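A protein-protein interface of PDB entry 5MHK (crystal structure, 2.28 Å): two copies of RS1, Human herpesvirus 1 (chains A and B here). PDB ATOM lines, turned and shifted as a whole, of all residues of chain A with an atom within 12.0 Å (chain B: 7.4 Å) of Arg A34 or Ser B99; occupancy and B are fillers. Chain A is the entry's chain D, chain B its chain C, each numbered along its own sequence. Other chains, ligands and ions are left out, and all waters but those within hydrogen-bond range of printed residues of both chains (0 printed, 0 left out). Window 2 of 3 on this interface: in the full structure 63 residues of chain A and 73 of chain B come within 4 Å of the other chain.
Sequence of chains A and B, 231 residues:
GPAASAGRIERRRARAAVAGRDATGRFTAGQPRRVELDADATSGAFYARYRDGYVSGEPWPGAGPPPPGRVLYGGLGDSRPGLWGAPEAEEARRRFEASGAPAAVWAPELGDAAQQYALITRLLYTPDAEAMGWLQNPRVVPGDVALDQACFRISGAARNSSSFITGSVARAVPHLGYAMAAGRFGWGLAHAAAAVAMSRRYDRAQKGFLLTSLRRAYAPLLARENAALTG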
ATOM      1  N   ARG A  33     -14.797  25.323  12.006  1.00  0.00           N
ATOM      2  CA  ARG A  33     -13.595  24.506  11.884  1.00  0.00           C
ATOM      3  C   ARG A  33     -13.250  23.826  13.206  1.00  0.00           C
ATOM      4  O   ARG A  33     -14.107  23.673  14.076  1.00  0.00           O
ATOM      5  CB  ARG A  33     -12.416  25.356  11.405  1.00  0.00           C
ATOM      6  CG  ARG A  33     -12.585  25.907  10.000  1.00  0.00           C
ATOM      7  CD  ARG A  33     -11.245  26.310   9.411  1.00  0.00           C
ATOM      8  NE  ARG A  33     -10.259  25.244   9.559  1.00  0.00           N
ATOM      9  CZ  ARG A  33      -9.064  25.241   8.977  1.00  0.00           C
ATOM     10  NH1 ARG A  33      -8.701  26.249   8.197  1.00  0.00           N
ATOM     11  NH2 ARG A  33      -8.233  24.226   9.174  1.00  0.00           N
ATOM     12  N   ARG A  34     -11.990  23.422  13.352  1.00  0.00           N
ATOM     13  CA  ARG A  34     -11.553  22.688  14.530  1.00  0.00           C
ATOM     14  C   ARG A  34     -10.037  22.770  14.634  1.00  0.00           C
ATOM     15  O   ARG A  34      -9.336  22.852  13.622  1.00  0.00           O
ATOM     16  CB  ARG A  34     -12.009  21.226  14.472  1.00  0.00           C
ATOM     17  CG  ARG A  34     -11.887  20.468  15.784  1.00  0.00           C
ATOM     18  CD  ARG A  34     -12.156  18.989  15.575  1.00  0.00           C
ATOM     19  NE  ARG A  34     -12.289  18.265  16.836  1.00  0.00           N
ATOM     20  CZ  ARG A  34     -12.427  16.947  16.927  1.00  0.00           C
ATOM     21  NH1 ARG A  34     -12.446  16.204  15.829  1.00  0.00           N
ATOM     22  NH2 ARG A  34     -12.545  16.370  18.116  1.00  0.00           N
ATOM     23  N   VAL A  35      -9.541  22.745  15.870  1.00  0.00           N
ATOM     24  CA  VAL A  35      -8.117  22.844  16.164  1.00  0.00           C
ATOM     25  C   VAL A  35      -7.700  21.613  16.954  1.00  0.00           C
ATOM     26  O   VAL A  35      -8.291  21.311  17.997  1.00  0.00           O
ATOM     27  CB  VAL A  35      -7.787  24.129  16.944  1.00  0.00           C
ATOM     28  CG1 VAL A  35      -6.326  24.142  17.354  1.00  0.00           C
ATOM     29  CG2 VAL A  35      -8.117  25.348  16.109  1.00  0.00           C
ATOM     30  N   GLU A  36      -6.678  20.913  16.469  1.00  0.00           N
ATOM     31  CA  GLU A  36      -6.196  19.684  17.093  1.00  0.00           C
ATOM     32  C   GLU A  36      -4.890  19.971  17.823  1.00  0.00           C
ATOM     33  O   GLU A  36      -3.864  20.245  17.190  1.00  0.00           O
ATOM     34  CB  GLU A  36      -6.014  18.580  16.054  1.00  0.00           C
ATOM     35  CG  GLU A  36      -7.318  17.957  15.594  1.00  0.00           C
ATOM     36  CD  GLU A  36      -8.087  17.322  16.736  1.00  0.00           C
ATOM     37  OE1 GLU A  36      -7.446  16.741  17.638  1.00  0.00           O
ATOM     38  OE2 GLU A  36      -9.334  17.409  16.737  1.00  0.00           O
ATOM     39  N   LEU A  37      -4.930  19.908  19.151  1.00  0.00           N
ATOM     40  CA  LEU A  37      -3.721  20.027  19.949  1.00  0.00           C
ATOM     41  C   LEU A  37      -2.978  18.700  19.975  1.00  0.00           C
ATOM     42  O   LEU A  37      -3.589  17.627  19.988  1.00  0.00           O
ATOM     43  CB  LEU A  37      -4.052  20.467  21.376  1.00  0.00           C
ATOM     44  CG  LEU A  37      -4.439  21.933  21.570  1.00  0.00           C
ATOM     45  CD1 LEU A  37      -4.651  22.241  23.043  1.00  0.00           C
ATOM     46  CD2 LEU A  37      -3.388  22.855  20.972  1.00  0.00           C
ATOM     47  N   ASP A  38      -1.651  18.780  19.981  1.00  0.00           N
ATOM     48  CA  ASP A  38      -0.809  17.594  19.988  1.00  0.00           C
ATOM     49  C   ASP A  38       0.531  17.951  20.612  1.00  0.00           C
ATOM     50  O   ASP A  38       0.810  19.114  20.913  1.00  0.00           O
ATOM     51  CB  ASP A  38      -0.631  17.031  18.573  1.00  0.00           C
ATOM     52  CG  ASP A  38      -0.437  18.118  17.533  1.00  0.00           C
ATOM     53  OD1 ASP A  38       0.581  18.840  17.604  1.00  0.00           O
ATOM     54  OD2 ASP A  38      -1.303  18.252  16.643  1.00  0.00           O
ATOM     55  N   ALA A  41       2.728  20.783  18.969  1.00  0.00           N
ATOM     56  CA  ALA A  41       2.502  22.170  19.356  1.00  0.00           C
ATOM     57  C   ALA A  41       2.677  22.397  20.851  1.00  0.00           C
ATOM     58  O   ALA A  41       3.105  23.484  21.257  1.00  0.00           O
ATOM     59  CB  ALA A  41       1.100  22.616  18.931  1.00  0.00           C
ATOM     60  N   PHE A  46       6.121  22.895  16.798  1.00  0.00           N
ATOM     61  CA  PHE A  46       5.390  23.393  15.639  1.00  0.00           C
ATOM     62  C   PHE A  46       5.692  24.865  15.403  1.00  0.00           C
ATOM     63  O   PHE A  46       5.701  25.324  14.255  1.00  0.00           O
ATOM     64  CB  PHE A  46       3.888  23.183  15.827  1.00  0.00           C
ATOM     65  CG  PHE A  46       3.041  23.928  14.830  1.00  0.00           C
ATOM     66  CD1 PHE A  46       2.804  23.400  13.572  1.00  0.00           C
ATOM     67  CD2 PHE A  46       2.483  25.156  15.153  1.00  0.00           C
ATOM     68  CE1 PHE A  46       2.029  24.083  12.653  1.00  0.00           C
ATOM     69  CE2 PHE A  46       1.709  25.844  14.238  1.00  0.00           C
ATOM     70  CZ  PHE A  46       1.480  25.307  12.987  1.00  0.00           C
ATOM     71  N   TYR A  47       5.949  25.608  16.478  1.00  0.00           N
ATOM     72  CA  TYR A  47       6.272  27.024  16.379  1.00  0.00           C
ATOM     73  C   TYR A  47       7.723  27.239  15.970  1.00  0.00           C
ATOM     74  O   TYR A  47       8.038  28.244  15.322  1.00  0.00           O
ATOM     75  CB  TYR A  47       5.939  27.716  17.702  1.00  0.00           C
ATOM     76  CG  TYR A  47       4.486  27.528  18.081  1.00  0.00           C
ATOM     77  CD1 TYR A  47       3.480  28.188  17.385  1.00  0.00           C
ATOM     78  CD2 TYR A  47       4.115  26.661  19.100  1.00  0.00           C
ATOM     79  CE1 TYR A  47       2.149  28.012  17.710  1.00  0.00           C
ATOM     80  CE2 TYR A  47       2.783  26.476  19.433  1.00  0.00           C
ATOM     81  CZ  TYR A  47       1.805  27.155  18.734  1.00  0.00           C
ATOM     82  OH  TYR A  47       0.478  26.978  19.058  1.00  0.00           O
ATOM     83  N   ALA B  92     -22.240  24.808  28.877  1.00  0.00           N
ATOM     84  CA  ALA B  92     -21.136  25.234  28.027  1.00  0.00           C
ATOM     85  C   ALA B  92     -19.897  24.369  28.235  1.00  0.00           C
ATOM     86  O   ALA B  92     -19.129  24.160  27.291  1.00  0.00           O
ATOM     87  CB  ALA B  92     -20.810  26.704  28.286  1.00  0.00           C
ATOM     88  N   ARG B  93     -19.681  23.872  29.458  1.00  0.00           N
ATOM     89  CA  ARG B  93     -18.533  23.004  29.704  1.00  0.00           C
ATOM     90  C   ARG B  93     -18.629  21.722  28.886  1.00  0.00           C
ATOM     91  O   ARG B  93     -17.636  21.272  28.303  1.00  0.00           O
ATOM     92  CB  ARG B  93     -18.423  22.675  31.194  1.00  0.00           C
ATOM     93  CG  ARG B  93     -17.206  21.825  31.539  1.00  0.00           C
ATOM     94  CD  ARG B  93     -17.013  21.672  33.041  1.00  0.00           C
ATOM     95  NE  ARG B  93     -17.985  20.748  33.622  1.00  0.00           N
ATOM     96  CZ  ARG B  93     -17.820  19.430  33.675  1.00  0.00           C
ATOM     97  NH1 ARG B  93     -16.723  18.875  33.179  1.00  0.00           N
ATOM     98  NH2 ARG B  93     -18.755  18.665  34.221  1.00  0.00           N
ATOM     99  N   ARG B  94     -19.818  21.118  28.838  1.00  0.00           N
ATOM    100  CA  ARG B  94     -20.003  19.898  28.061  1.00  0.00           C
ATOM    101  C   ARG B  94     -19.789  20.146  26.573  1.00  0.00           C
ATOM    102  O   ARG B  94     -19.124  19.352  25.895  1.00  0.00           O
ATOM    103  CB  ARG B  94     -21.394  19.326  28.327  1.00  0.00           C
ATOM    104  CG  ARG B  94     -21.567  18.803  29.745  1.00  0.00           C
ATOM    105  CD  ARG B  94     -22.904  18.109  29.933  1.00  0.00           C
ATOM    106  NE  ARG B  94     -23.066  17.624  31.301  1.00  0.00           N
ATOM    107  CZ  ARG B  94     -23.674  18.296  32.273  1.00  0.00           C
ATOM    108  NH1 ARG B  94     -24.178  19.499  32.040  1.00  0.00           N
ATOM    109  NH2 ARG B  94     -23.768  17.762  33.484  1.00  0.00           N
ATOM    110  N   ARG B  95     -20.351  21.237  26.044  1.00  0.00           N
ATOM    111  CA  ARG B  95     -20.141  21.572  24.639  1.00  0.00           C
ATOM    112  C   ARG B  95     -18.665  21.788  24.331  1.00  0.00           C
ATOM    113  O   ARG B  95     -18.170  21.348  23.286  1.00  0.00           O
ATOM    114  CB  ARG B  95     -20.955  22.808  24.258  1.00  0.00           C
ATOM    115  CG  ARG B  95     -22.390  22.505  23.865  1.00  0.00           C
ATOM    116  CD  ARG B  95     -23.060  23.708  23.220  1.00  0.00           C
ATOM    117  NE  ARG B  95     -23.189  24.836  24.137  1.00  0.00           N
ATOM    118  CZ  ARG B  95     -22.459  25.945  24.063  1.00  0.00           C
ATOM    119  NH1 ARG B  95     -21.546  26.077  23.110  1.00  0.00           N
ATOM    120  NH2 ARG B  95     -22.645  26.923  24.939  1.00  0.00           N
ATOM    121  N   PHE B  96     -17.946  22.466  25.228  1.00  0.00           N
ATOM    122  CA  PHE B  96     -16.525  22.721  25.010  1.00  0.00           C
ATOM    123  C   PHE B  96     -15.735  21.420  24.950  1.00  0.00           C
ATOM    124  O   PHE B  96     -14.886  21.234  24.070  1.00  0.00           O
ATOM    125  CB  PHE B  96     -15.985  23.631  26.113  1.00  0.00           C
ATOM    126  CG  PHE B  96     -14.503  23.863  26.038  1.00  0.00           C
ATOM    127  CD1 PHE B  96     -13.931  24.430  24.911  1.00  0.00           C
ATOM    128  CD2 PHE B  96     -13.682  23.515  27.098  1.00  0.00           C
ATOM    129  CE1 PHE B  96     -12.567  24.644  24.841  1.00  0.00           C
ATOM    130  CE2 PHE B  96     -12.316  23.727  27.034  1.00  0.00           C
ATOM    131  CZ  PHE B  96     -11.758  24.292  25.905  1.00  0.00           C
ATOM    132  N   GLU B  97     -16.003  20.502  25.881  1.00  0.00           N
ATOM    133  CA  GLU B  97     -15.250  19.256  25.943  1.00  0.00           C
ATOM    134  C   GLU B  97     -15.573  18.316  24.789  1.00  0.00           C
ATOM    135  O   GLU B  97     -14.786  17.405  24.510  1.00  0.00           O
ATOM    136  CB  GLU B  97     -15.521  18.552  27.274  1.00  0.00           C
ATOM    137  CG  GLU B  97     -14.986  19.294  28.487  1.00  0.00           C
ATOM    138  CD  GLU B  97     -15.148  18.504  29.770  1.00  0.00           C
ATOM    139  OE1 GLU B  97     -15.071  17.259  29.716  1.00  0.00           O
ATOM    140  OE2 GLU B  97     -15.356  19.128  30.832  1.00  0.00           O
ATOM    141  N   ALA B  98     -16.703  18.515  24.111  1.00  0.00           N
ATOM    142  CA  ALA B  98     -17.142  17.621  23.049  1.00  0.00           C
ATOM    143  C   ALA B  98     -16.823  18.131  21.649  1.00  0.00           C
ATOM    144  O   ALA B  98     -17.002  17.384  20.682  1.00  0.00           O
ATOM    145  CB  ALA B  98     -18.651  17.368  23.161  1.00  0.00           C
ATOM    146  N   SER B  99     -16.360  19.372  21.514  1.00  0.00           N
ATOM    147  CA  SER B  99     -16.156  19.975  20.203  1.00  0.00           C
ATOM    148  C   SER B  99     -14.729  19.842  19.693  1.00  0.00           C
ATOM    149  O   SER B  99     -14.520  19.805  18.475  1.00  0.00           O
ATOM    150  CB  SER B  99     -16.537  21.459  20.235  1.00  0.00           C
ATOM    151  OG  SER B  99     -15.667  22.193  21.078  1.00  0.00           O
ATOM    152  N   GLY B 100     -13.745  19.772  20.587  1.00  0.00           N
ATOM    153  CA  GLY B 100     -12.354  19.781  20.188  1.00  0.00           C
ATOM    154  C   GLY B 100     -11.857  21.091  19.624  1.00  0.00           C
ATOM    155  O   GLY B 100     -10.700  21.161  19.197  1.00  0.00           O
ATOM    156  N   ALA B 101     -12.683  22.126  19.608  1.00  0.00           N
ATOM    157  CA  ALA B 101     -12.333  23.448  19.123  1.00  0.00           C
ATOM    158  C   ALA B 101     -12.318  24.442  20.277  1.00  0.00           C
ATOM    159  O   ALA B 101     -12.912  24.191  21.331  1.00  0.00           O
ATOM    160  CB  ALA B 101     -13.333  23.907  18.052  1.00  0.00           C
ATOM    161  N   PRO B 102     -11.633  25.576  20.126  1.00  0.00           N
ATOM    162  CA  PRO B 102     -11.687  26.595  21.179  1.00  0.00           C
ATOM    163  C   PRO B 102     -13.099  27.141  21.320  1.00  0.00           C
ATOM    164  O   PRO B 102     -13.807  27.346  20.331  1.00  0.00           O
ATOM    165  CB  PRO B 102     -10.707  27.669  20.689  1.00  0.00           C
ATOM    166  CG  PRO B 102     -10.607  27.452  19.216  1.00  0.00           C
ATOM    167  CD  PRO B 102     -10.738  25.973  19.024  1.00  0.00           C
ATOM    168  N   ALA B 103     -13.509  27.369  22.564  1.00  0.00           N
ATOM    169  CA  ALA B 103     -14.845  27.886  22.818  1.00  0.00           C
ATOM    170  C   ALA B 103     -14.954  29.335  22.361  1.00  0.00           C
ATOM    171  O   ALA B 103     -14.033  30.135  22.551  1.00  0.00           O
ATOM    172  CB  ALA B 103     -15.184  27.775  24.304  1.00  0.00           C
ATOM    173  N   LEU B 119      -5.272  26.309  22.449  1.00  0.00           N
ATOM    174  CA  LEU B 119      -6.132  26.131  21.282  1.00  0.00           C
ATOM    175  C   LEU B 119      -6.210  27.406  20.452  1.00  0.00           C
ATOM    176  O   LEU B 119      -6.168  27.351  19.217  1.00  0.00           O
ATOM    177  CB  LEU B 119      -7.532  25.696  21.717  1.00  0.00           C
ATOM    178  CG  LEU B 119      -7.718  24.268  22.229  1.00  0.00           C
ATOM    179  CD1 LEU B 119      -9.028  24.145  22.987  1.00  0.00           C
ATOM    180  CD2 LEU B 119      -7.695  23.299  21.062  1.00  0.00           C
ATOM    181  N   LEU B 123      -4.727  28.007  16.765  1.00  0.00           N
ATOM    182  CA  LEU B 123      -5.650  28.515  15.753  1.00  0.00           C
ATOM    183  C   LEU B 123      -5.064  29.710  15.016  1.00  0.00           C
ATOM    184  O   LEU B 123      -5.277  29.870  13.808  1.00  0.00           O
ATOM    185  CB  LEU B 123      -6.982  28.890  16.404  1.00  0.00           C
ATOM    186  CG  LEU B 123      -8.068  29.490  15.507  1.00  0.00           C
ATOM    187  CD1 LEU B 123      -8.556  28.487  14.476  1.00  0.00           C
ATOM    188  CD2 LEU B 123      -9.226  29.996  16.349  1.00  0.00           C
ATOM    189  N   THR B 126      -2.994  28.403  12.043  1.00  0.00           N
ATOM    190  CA  THR B 126      -3.440  27.480  10.996  1.00  0.00           C
ATOM    191  C   THR B 126      -3.935  28.273   9.794  1.00  0.00           C
ATOM    192  O   THR B 126      -4.748  29.190   9.960  1.00  0.00           O
ATOM    193  CB  THR B 126      -4.545  26.543  11.474  1.00  0.00           C
ATOM    194  OG1 THR B 126      -5.818  27.049  11.062  1.00  0.00           O
ATOM    195  CG2 THR B 126      -4.537  26.397  12.971  1.00  0.00           C
ATOM    196  N   ALA B 129      -7.908  29.723   8.610  1.00  0.00           N
ATOM    197  CA  ALA B 129      -8.737  29.539   9.797  1.00  0.00           C
ATOM    198  C   ALA B 129      -9.653  30.719  10.095  1.00  0.00           C
ATOM    199  O   ALA B 129     -10.588  30.567  10.888  1.00  0.00           O
ATOM    200  CB  ALA B 129      -7.856  29.286  11.021  1.00  0.00           C
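The backbone carbonyl oxygen of Gly B100 lies close to the backbone carbonyl oxygen of Val A35 (2.7 Å).
O of Ser B99 is in hydrogen-bond range of NE of Arg A34 (3.2 Å).
Printed residues of chain B within 4 Å of Arg A34: Ser B99 (3.2 Å) and Gly B100 (3.7 Å).
Of the printed residues of chain B, Val A35 touches Gly B100 (2.7 Å), Pro B102 (3.97 Å), Leu B119 (3.7 Å) and Leu B123 (3.6 Å).
Printed residues of chain B within 4 Å of Leu A37: Leu B119.
Tyr A47 touches none of the printed residues of chain B.
No residue of chain A comes within 4 Å of Phe B96.
No residue of chain A comes within 4 Å of Ala B98.
Of chain A, only Arg A34 comes within 4 Å of Ser B99.
Gly B100 touches just these residues of chain A: Arg A34 and Val A35.
No residue of chain A comes within 4 Å of Ala B101.
Printed residues of chain A within 4 Å of Leu B119: Val A35 and Leu A37.
Thr B126 touches none of the printed residues of chain A.
Of the printed residues of chain A, Ala B129 touches Arg A33 (3.6 Å).
The nearest residue of chain A that does not touch Ser B99 is Arg A33 (5.9 Å).
No position is printed for both chains.
Of the 8 pairs that touch across the chains among the printed residues, none has its exchanged pair printed and touching as well.
Hydrophobic or aromatic side chains of chain B within 4 Å of the printed part of chain A: Pro B102, Leu B119 and Leu B123.
Of the 9 printed residues of chain A, 4 touch a printed residue of chain B.
Printed residues of chain A that touch a printed residue of chain B: Arg A33, Arg A34, Val A35 and Leu A37.
Hydrophobic or aromatic side chains of chain A within 4 Å of the printed part of chain B: Val A35 and Leu A37.
Among the printed residues, no Asp or Glu carboxylate lies within 4 Å of a Lys or Arg side-chain nitrogen of the other chain.
The backbone carbonyl oxygen of Arg B95 lies within hydrogen-bond range of the side-chain hydroxyl of Ser B99, 3.4 Å away.
The side-chain hydroxyl (OG) of Ser B99 sits close to the backbone NH (N) of Ala B101, at 3.3 Å.
The backbone carbonyl oxygen of Phe B96 sits at hydrogen-bond distance from the side-chain hydroxyl of Ser B99, 3.2 Å away.
The guanidinium group of Arg A34 is in salt-bridge range of the side-chain carboxylate of Glu A36.
Arg A33 touches Ala B129.
Arg A34 touches Gly B100.
Val A35 touches Pro B102.
Val A35 touches Leu B119 (O to CD2, 3.7 Å).
CG2 of Val A35 touches CD1 of Leu B123, 3.6 Å away.
CG of Leu A37 touches CD2 of Leu B119 (3.6 Å).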
